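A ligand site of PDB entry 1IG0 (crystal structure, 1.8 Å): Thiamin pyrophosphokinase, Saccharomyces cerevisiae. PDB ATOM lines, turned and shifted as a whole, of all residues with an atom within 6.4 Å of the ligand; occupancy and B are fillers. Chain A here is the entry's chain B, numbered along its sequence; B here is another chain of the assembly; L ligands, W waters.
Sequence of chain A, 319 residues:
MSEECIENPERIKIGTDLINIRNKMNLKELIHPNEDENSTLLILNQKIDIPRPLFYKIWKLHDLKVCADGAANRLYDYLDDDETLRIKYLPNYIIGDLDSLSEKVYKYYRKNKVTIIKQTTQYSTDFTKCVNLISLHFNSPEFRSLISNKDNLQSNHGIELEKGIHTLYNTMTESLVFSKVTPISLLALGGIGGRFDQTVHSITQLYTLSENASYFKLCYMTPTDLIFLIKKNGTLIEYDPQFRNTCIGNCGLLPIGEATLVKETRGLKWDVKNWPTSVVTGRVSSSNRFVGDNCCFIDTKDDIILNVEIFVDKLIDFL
O of Gln 122 of chain B lies within hydrogen-bond range of N1 of the ligand (3.0 Å).
OG of Ser 285 sits at hydrogen-bond distance from N4 of the ligand (2.7 Å).
ND2 of Asn 288 lies within hydrogen-bond range of N4 of the ligand (3.5 Å).
N of Ser 124 of chain B lies close to S1 of the ligand (3.8 Å).
A sulfur (S1) of the ligand sits close to the backbone NH (N) of Thr 125 of chain B, at 3.6 Å.
An oxygen (O1) of the ligand is in hydrogen-bond range of the side-chain hydroxyl (OG) of Ser 287, at 3.4 Å.
OG of Ser 287 lies within hydrogen-bond range of NE2 of Gln 198 of chain B (3.4 Å).
OG of Ser 285 is in hydrogen-bond range of ND2 of Asn 288 (2.8 Å).
The side-chain hydroxyl (OH) of Tyr 123 of chain B lies within hydrogen-bond range of the side-chain carboxylate (OE1) of Glu 7 (2.9 Å).
The side-chain amide nitrogen (ND2) of Asn 288 sits at hydrogen-bond distance from the backbone carbonyl oxygen (O) of Trp 270.
The side-chain hydroxyl (OH) of Tyr 123 of chain B is in hydrogen-bond range of the indole nitrogen (NE1) of Trp 270 (3.2 Å).
N of Tyr 123 of chain B lies within hydrogen-bond range of OG1 of Thr 121 of chain B (3.2 Å).
The indole nitrogen (NE1) of Trp 270 is in hydrogen-bond range of the side-chain carboxylate (OE1) of Glu 7, at 3.2 Å.
The indole nitrogen (NE1) of Trp 270 sits close to a nitrogen (N1) of the ligand, 3.5 Å away.
N2 of the ligand lies close to O of Ser 286.
Cys 5 touches the ligand.
Val 272 touches the ligand.
Trp 275 touches the ligand.
Tyr 123 of chain B touches the ligand.
Hydrophobic or aromatic side chains that line the ligand: Trp 270, Val 272, Trp 275 and Tyr 123 of chain B.
12 residues have an atom within 4 Å of the ligand: Cys 5, Trp 270, Val 272, Trp 275, Ser 285, Ser 286, Ser 287, Asn 288, Gln 122 of chain B, Tyr 123 of chain B, Ser 124 of chain B and Thr 125 of chain B.
The nearest printed residue that does not touch the ligand is Gln 198 of chain B (4.1 Å).
Water W2 bridges O1 of the ligand (3.0 Å) and N of Asp 126 of chain B (3.2 Å).
Water W4 bridges a sulfur (S1) of the ligand (3.2 Å) and the backbone carbonyl oxygen of Tyr 123 of chain B (3.4 Å).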
ATOM      1  N   CYS A   5      13.191  31.186  11.136  1.00  0.00           N
ATOM      2  CA  CYS A   5      12.646  29.891  10.738  1.00  0.00           C
ATOM      3  C   CYS A   5      13.192  29.607   9.353  1.00  0.00           C
ATOM      4  O   CYS A   5      13.006  30.407   8.433  1.00  0.00           O
ATOM      5  CB  CYS A   5      11.122  29.938  10.698  1.00  0.00           C
ATOM      6  SG  CYS A   5      10.360  28.414  10.078  1.00  0.00           S
ATOM      7  N   GLU A   7      13.801  26.603   6.157  1.00  0.00           N
ATOM      8  CA  GLU A   7      13.347  25.341   5.592  1.00  0.00           C
ATOM      9  C   GLU A   7      14.560  24.594   5.076  1.00  0.00           C
ATOM     10  O   GLU A   7      15.204  25.025   4.116  1.00  0.00           O
ATOM     11  CB  GLU A   7      12.355  25.592   4.456  1.00  0.00           C
ATOM     12  CG  GLU A   7      11.658  24.327   3.977  1.00  0.00           C
ATOM     13  CD  GLU A   7      10.600  24.614   2.930  1.00  0.00           C
ATOM     14  OE1 GLU A   7       9.739  25.482   3.178  1.00  0.00           O
ATOM     15  OE2 GLU A   7      10.633  23.960   1.869  1.00  0.00           O
ATOM     16  N   TRP A 270      11.894  22.207   9.350  1.00  0.00           N
ATOM     17  CA  TRP A 270      11.738  23.630   9.611  1.00  0.00           C
ATOM     18  C   TRP A 270      12.373  23.914  10.967  1.00  0.00           C
ATOM     19  O   TRP A 270      11.758  23.674  12.013  1.00  0.00           O
ATOM     20  CB  TRP A 270      10.257  24.001   9.628  1.00  0.00           C
ATOM     21  CG  TRP A 270       9.633  24.015   8.264  1.00  0.00           C
ATOM     22  CD1 TRP A 270       9.645  25.034   7.355  1.00  0.00           C
ATOM     23  CD2 TRP A 270       8.927  22.926   7.637  1.00  0.00           C
ATOM     24  NE1 TRP A 270       8.994  24.660   6.202  1.00  0.00           N
ATOM     25  CE2 TRP A 270       8.551  23.371   6.347  1.00  0.00           C
ATOM     26  CE3 TRP A 270       8.595  21.628   8.037  1.00  0.00           C
ATOM     27  CZ2 TRP A 270       7.840  22.559   5.455  1.00  0.00           C
ATOM     28  CZ3 TRP A 270       7.884  20.817   7.145  1.00  0.00           C
ATOM     29  CH2 TRP A 270       7.524  21.284   5.865  1.00  0.00           C
ATOM     30  N   ASP A 271      13.613  24.393  10.944  1.00  0.00           N
ATOM     31  CA  ASP A 271      14.336  24.719  12.177  1.00  0.00           C
ATOM     32  C   ASP A 271      14.044  26.154  12.578  1.00  0.00           C
ATOM     33  O   ASP A 271      13.905  27.032  11.732  1.00  0.00           O
ATOM     34  CB  ASP A 271      15.840  24.546  11.996  1.00  0.00           C
ATOM     35  CG  ASP A 271      16.296  23.101  12.188  1.00  0.00           C
ATOM     36  OD1 ASP A 271      15.717  22.406  13.039  1.00  0.00           O
ATOM     37  OD2 ASP A 271      17.246  22.677  11.496  1.00  0.00           O
ATOM     38  N   VAL A 272      13.959  26.384  13.882  1.00  0.00           N
ATOM     39  CA  VAL A 272      13.676  27.720  14.406  1.00  0.00           C
ATOM     40  C   VAL A 272      14.690  28.181  15.440  1.00  0.00           C
ATOM     41  O   VAL A 272      15.457  27.383  15.977  1.00  0.00           O
ATOM     42  CB  VAL A 272      12.266  27.779  15.021  1.00  0.00           C
ATOM     43  CG1 VAL A 272      11.219  27.470  13.965  1.00  0.00           C
ATOM     44  CG2 VAL A 272      12.148  26.779  16.157  1.00  0.00           C
ATOM     45  N   TRP A 275      12.260  31.450  18.776  1.00  0.00           N
ATOM     46  CA  TRP A 275      10.906  31.278  18.257  1.00  0.00           C
ATOM     47  C   TRP A 275       9.871  31.050  19.351  1.00  0.00           C
ATOM     48  O   TRP A 275       9.781  29.952  19.908  1.00  0.00           O
ATOM     49  CB  TRP A 275      10.925  30.089  17.300  1.00  0.00           C
ATOM     50  CG  TRP A 275       9.841  30.042  16.277  1.00  0.00           C
ATOM     51  CD1 TRP A 275       9.795  30.732  15.103  1.00  0.00           C
ATOM     52  CD2 TRP A 275       8.679  29.214  16.305  1.00  0.00           C
ATOM     53  NE1 TRP A 275       8.676  30.380  14.390  1.00  0.00           N
ATOM     54  CE2 TRP A 275       7.974  29.451  15.110  1.00  0.00           C
ATOM     55  CE3 TRP A 275       8.153  28.292  17.226  1.00  0.00           C
ATOM     56  CZ2 TRP A 275       6.771  28.802  14.795  1.00  0.00           C
ATOM     57  CZ3 TRP A 275       6.963  27.644  16.919  1.00  0.00           C
ATOM     58  CH2 TRP A 275       6.284  27.904  15.717  1.00  0.00           C
ATOM     59  N   VAL A 284       2.490  27.091  16.834  1.00  0.00           N
ATOM     60  CA  VAL A 284       2.883  25.735  17.197  1.00  0.00           C
ATOM     61  C   VAL A 284       3.430  25.012  15.970  1.00  0.00           C
ATOM     62  O   VAL A 284       2.796  24.991  14.916  1.00  0.00           O
ATOM     63  CB  VAL A 284       1.674  24.930  17.735  1.00  0.00           C
ATOM     64  CG1 VAL A 284       2.071  23.492  18.008  1.00  0.00           C
ATOM     65  CG2 VAL A 284       1.146  25.579  19.009  1.00  0.00           C
ATOM     66  N   SER A 285       4.606  24.410  16.121  1.00  0.00           N
ATOM     67  CA  SER A 285       5.233  23.684  15.037  1.00  0.00           C
ATOM     68  C   SER A 285       4.567  22.322  14.848  1.00  0.00           C
ATOM     69  O   SER A 285       4.880  21.362  15.556  1.00  0.00           O
ATOM     70  CB  SER A 285       6.728  23.497  15.296  1.00  0.00           C
ATOM     71  OG  SER A 285       7.351  22.842  14.208  1.00  0.00           O
ATOM     72  N   SER A 286       3.631  22.246  13.915  1.00  0.00           N
ATOM     73  CA  SER A 286       2.929  21.005  13.632  1.00  0.00           C
ATOM     74  C   SER A 286       3.311  20.540  12.243  1.00  0.00           C
ATOM     75  O   SER A 286       3.704  21.351  11.406  1.00  0.00           O
ATOM     76  CB  SER A 286       1.412  21.194  13.735  1.00  0.00           C
ATOM     77  OG  SER A 286       0.944  22.147  12.793  1.00  0.00           O
ATOM     78  N   SER A 287       3.199  19.244  11.993  1.00  0.00           N
ATOM     79  CA  SER A 287       3.558  18.689  10.696  1.00  0.00           C
ATOM     80  C   SER A 287       5.014  18.944  10.339  1.00  0.00           C
ATOM     81  O   SER A 287       5.349  19.154   9.171  1.00  0.00           O
ATOM     82  CB  SER A 287       2.648  19.259   9.595  1.00  0.00           C
ATOM     83  OG  SER A 287       1.328  18.781   9.721  1.00  0.00           O
ATOM     84  N   ASN A 288       5.884  18.934  11.339  1.00  0.00           N
ATOM     85  CA  ASN A 288       7.305  19.129  11.090  1.00  0.00           C
ATOM     86  C   ASN A 288       7.817  17.708  10.859  1.00  0.00           C
ATOM     87  O   ASN A 288       7.037  16.753  10.865  1.00  0.00           O
ATOM     88  CB  ASN A 288       7.999  19.743  12.314  1.00  0.00           C
ATOM     89  CG  ASN A 288       9.224  20.572  11.937  1.00  0.00           C
ATOM     90  OD1 ASN A 288       9.975  20.217  11.029  1.00  0.00           O
ATOM     91  ND2 ASN A 288       9.419  21.670  12.651  1.00  0.00           N
ATOM     92  N   ARG A 289       9.122  17.558  10.661  1.00  0.00           N
ATOM     93  CA  ARG A 289       9.682  16.226  10.446  1.00  0.00           C
ATOM     94  C   ARG A 289      11.193  16.263  10.618  1.00  0.00           C
ATOM     95  O   ARG A 289      11.822  17.314  10.437  1.00  0.00           O
ATOM     96  CB  ARG A 289       9.340  15.723   9.038  1.00  0.00           C
ATOM     97  CG  ARG A 289      10.215  16.310   7.935  1.00  0.00           C
ATOM     98  CD  ARG A 289       9.748  15.886   6.555  1.00  0.00           C
ATOM     99  NE  ARG A 289       8.513  16.550   6.180  1.00  0.00           N
ATOM    100  CZ  ARG A 289       8.343  17.213   5.036  1.00  0.00           C
ATOM    101  NH1 ARG A 289       9.332  17.300   4.162  1.00  0.00           N
ATOM    102  NH2 ARG A 289       7.173  17.781   4.772  1.00  0.00           N
ATOM    103  N   THR B 121       1.199  26.113  -0.306  1.00  0.00           N
ATOM    104  CA  THR B 121       1.945  26.551   0.870  1.00  0.00           C
ATOM    105  C   THR B 121       1.996  25.533   2.003  1.00  0.00           C
ATOM    106  O   THR B 121       0.972  24.980   2.405  1.00  0.00           O
ATOM    107  CB  THR B 121       1.400  27.873   1.445  1.00  0.00           C
ATOM    108  OG1 THR B 121       2.186  28.268   2.563  1.00  0.00           O
ATOM    109  CG2 THR B 121      -0.050  27.708   1.886  1.00  0.00           C
ATOM    110  N   GLN B 122       3.193  25.299   2.514  1.00  0.00           N
ATOM    111  CA  GLN B 122       3.399  24.374   3.624  1.00  0.00           C
ATOM    112  C   GLN B 122       3.600  25.153   4.908  1.00  0.00           C
ATOM    113  O   GLN B 122       4.173  24.641   5.873  1.00  0.00           O
ATOM    114  CB  GLN B 122       4.620  23.485   3.362  1.00  0.00           C
ATOM    115  CG  GLN B 122       4.483  22.531   2.189  1.00  0.00           C
ATOM    116  CD  GLN B 122       3.235  21.665   2.295  1.00  0.00           C
ATOM    117  OE1 GLN B 122       2.181  22.014   1.765  1.00  0.00           O
ATOM    118  NE2 GLN B 122       3.348  20.544   2.988  1.00  0.00           N
ATOM    119  N   TYR B 123       3.142  26.403   4.928  1.00  0.00           N
ATOM    120  CA  TYR B 123       3.279  27.251   6.102  1.00  0.00           C
ATOM    121  C   TYR B 123       1.946  27.495   6.797  1.00  0.00           C
ATOM    122  O   TYR B 123       1.865  28.255   7.756  1.00  0.00           O
ATOM    123  CB  TYR B 123       3.961  28.565   5.739  1.00  0.00           C
ATOM    124  CG  TYR B 123       5.446  28.396   5.522  1.00  0.00           C
ATOM    125  CD1 TYR B 123       5.941  27.897   4.320  1.00  0.00           C
ATOM    126  CD2 TYR B 123       6.338  28.644   6.556  1.00  0.00           C
ATOM    127  CE1 TYR B 123       7.295  27.645   4.153  1.00  0.00           C
ATOM    128  CE2 TYR B 123       7.704  28.393   6.396  1.00  0.00           C
ATOM    129  CZ  TYR B 123       8.170  27.900   5.200  1.00  0.00           C
ATOM    130  OH  TYR B 123       9.508  27.640   5.047  1.00  0.00           O
ATOM    131  N   SER B 124       0.904  26.853   6.286  1.00  0.00           N
ATOM    132  CA  SER B 124      -0.420  26.971   6.860  1.00  0.00           C
ATOM    133  C   SER B 124      -1.048  25.585   6.846  1.00  0.00           C
ATOM    134  O   SER B 124      -0.824  24.793   5.928  1.00  0.00           O
ATOM    135  CB  SER B 124      -1.291  27.927   6.047  1.00  0.00           C
ATOM    136  OG  SER B 124      -1.569  27.385   4.771  1.00  0.00           O
ATOM    137  N   THR B 125      -1.828  25.277   7.874  1.00  0.00           N
ATOM    138  CA  THR B 125      -2.478  23.979   7.963  1.00  0.00           C
ATOM    139  C   THR B 125      -3.702  23.987   7.053  1.00  0.00           C
ATOM    140  O   THR B 125      -4.153  25.051   6.611  1.00  0.00           O
ATOM    141  CB  THR B 125      -2.973  23.723   9.387  1.00  0.00           C
ATOM    142  OG1 THR B 125      -3.939  24.717   9.733  1.00  0.00           O
ATOM    143  CG2 THR B 125      -1.806  23.787  10.379  1.00  0.00           C
ATOM    144  N   ASP B 126      -4.234  22.805   6.768  1.00  0.00           N
ATOM    145  CA  ASP B 126      -5.418  22.726   5.929  1.00  0.00           C
ATOM    146  C   ASP B 126      -6.570  23.388   6.658  1.00  0.00           C
ATOM    147  O   ASP B 126      -7.474  23.940   6.041  1.00  0.00           O
ATOM    148  CB  ASP B 126      -5.763  21.270   5.597  1.00  0.00           C
ATOM    149  CG  ASP B 126      -4.787  20.649   4.619  1.00  0.00           C
ATOM    150  OD1 ASP B 126      -4.443  21.307   3.614  1.00  0.00           O
ATOM    151  OD2 ASP B 126      -4.381  19.493   4.835  1.00  0.00           O
ATOM    152  N   LYS B 129      -6.362  27.005   5.976  1.00  0.00           N
ATOM    153  CA  LYS B 129      -6.754  27.202   4.586  1.00  0.00           C
ATOM    154  C   LYS B 129      -8.267  27.205   4.507  1.00  0.00           C
ATOM    155  O   LYS B 129      -8.873  28.012   3.798  1.00  0.00           O
ATOM    156  CB  LYS B 129      -6.195  26.085   3.700  1.00  0.00           C
ATOM    157  CG  LYS B 129      -4.672  26.105   3.528  1.00  0.00           C
ATOM    158  CD  LYS B 129      -4.211  24.993   2.582  1.00  0.00           C
ATOM    159  CE  LYS B 129      -2.716  25.078   2.310  1.00  0.00           C
ATOM    160  NZ  LYS B 129      -1.895  24.891   3.527  1.00  0.00           N
ATOM    161  N   GLN B 198      -2.037  17.306  15.197  1.00  0.00           N
ATOM    162  CA  GLN B 198      -3.211  17.875  14.544  1.00  0.00           C
ATOM    163  C   GLN B 198      -4.285  18.160  15.584  1.00  0.00           C
ATOM    164  O   GLN B 198      -5.016  19.145  15.464  1.00  0.00           O
ATOM    165  CB  GLN B 198      -3.757  16.923  13.485  1.00  0.00           C
ATOM    166  CG  GLN B 198      -3.006  16.973  12.162  1.00  0.00           C
ATOM    167  CD  GLN B 198      -2.875  18.395  11.637  1.00  0.00           C
ATOM    168  OE1 GLN B 198      -3.856  19.133  11.568  1.00  0.00           O
ATOM    169  NE2 GLN B 198      -1.660  18.775  11.249  1.00  0.00           N
HETATM  170  C1  LIG L   1       8.080  26.204  12.477  1.00  0.00           C
HETATM  171  N1  LIG L   1       6.104  25.482   7.989  1.00  0.00           N
HETATM  172  C2  LIG L   1       4.008  21.044   6.617  1.00  0.00           C
HETATM  173  O1  LIG L   1      -0.417  21.317   8.237  1.00  0.00           O
HETATM  174  C3  LIG L   1       0.137  20.675   7.084  1.00  0.00           C
HETATM  175  C4  LIG L   1       1.010  21.689   6.302  1.00  0.00           C
HETATM  176  C5  LIG L   1       3.142  23.714   8.865  1.00  0.00           C
HETATM  177  S1  LIG L   1       1.430  23.726   8.347  1.00  0.00           S
HETATM  178  C6  LIG L   1       1.969  22.398   7.253  1.00  0.00           C
HETATM  179  C7  LIG L   1       3.294  22.118   7.409  1.00  0.00           C
HETATM  180  N2  LIG L   1       3.869  22.864   8.289  1.00  0.00           N
HETATM  181  C8  LIG L   1       5.319  22.764   8.636  1.00  0.00           C
HETATM  182  C9  LIG L   1       6.402  24.983   9.267  1.00  0.00           C
HETATM  183  N3  LIG L   1       7.069  25.808  10.202  1.00  0.00           N
HETATM  184  C10 LIG L   1       7.372  25.317  11.483  1.00  0.00           C
HETATM  185  N4  LIG L   1       7.013  24.007  11.832  1.00  0.00           N
HETATM  186  C11 LIG L   1       6.347  23.175  10.909  1.00  0.00           C
HETATM  187  C12 LIG L   1       6.039  23.659   9.625  1.00  0.00           C
HETATM  188  O   HOH W   1       6.479  28.674  10.085  1.00  0.00           O
HETATM  189  O   HOH W   2      -3.110  20.080   7.923  1.00  0.00           O
HETATM  190  O   HOH W   3       3.441  24.845  12.078  1.00  0.00           O
HETATM  191  O   HOH W   4       1.743  26.155  10.428  1.00  0.00           O
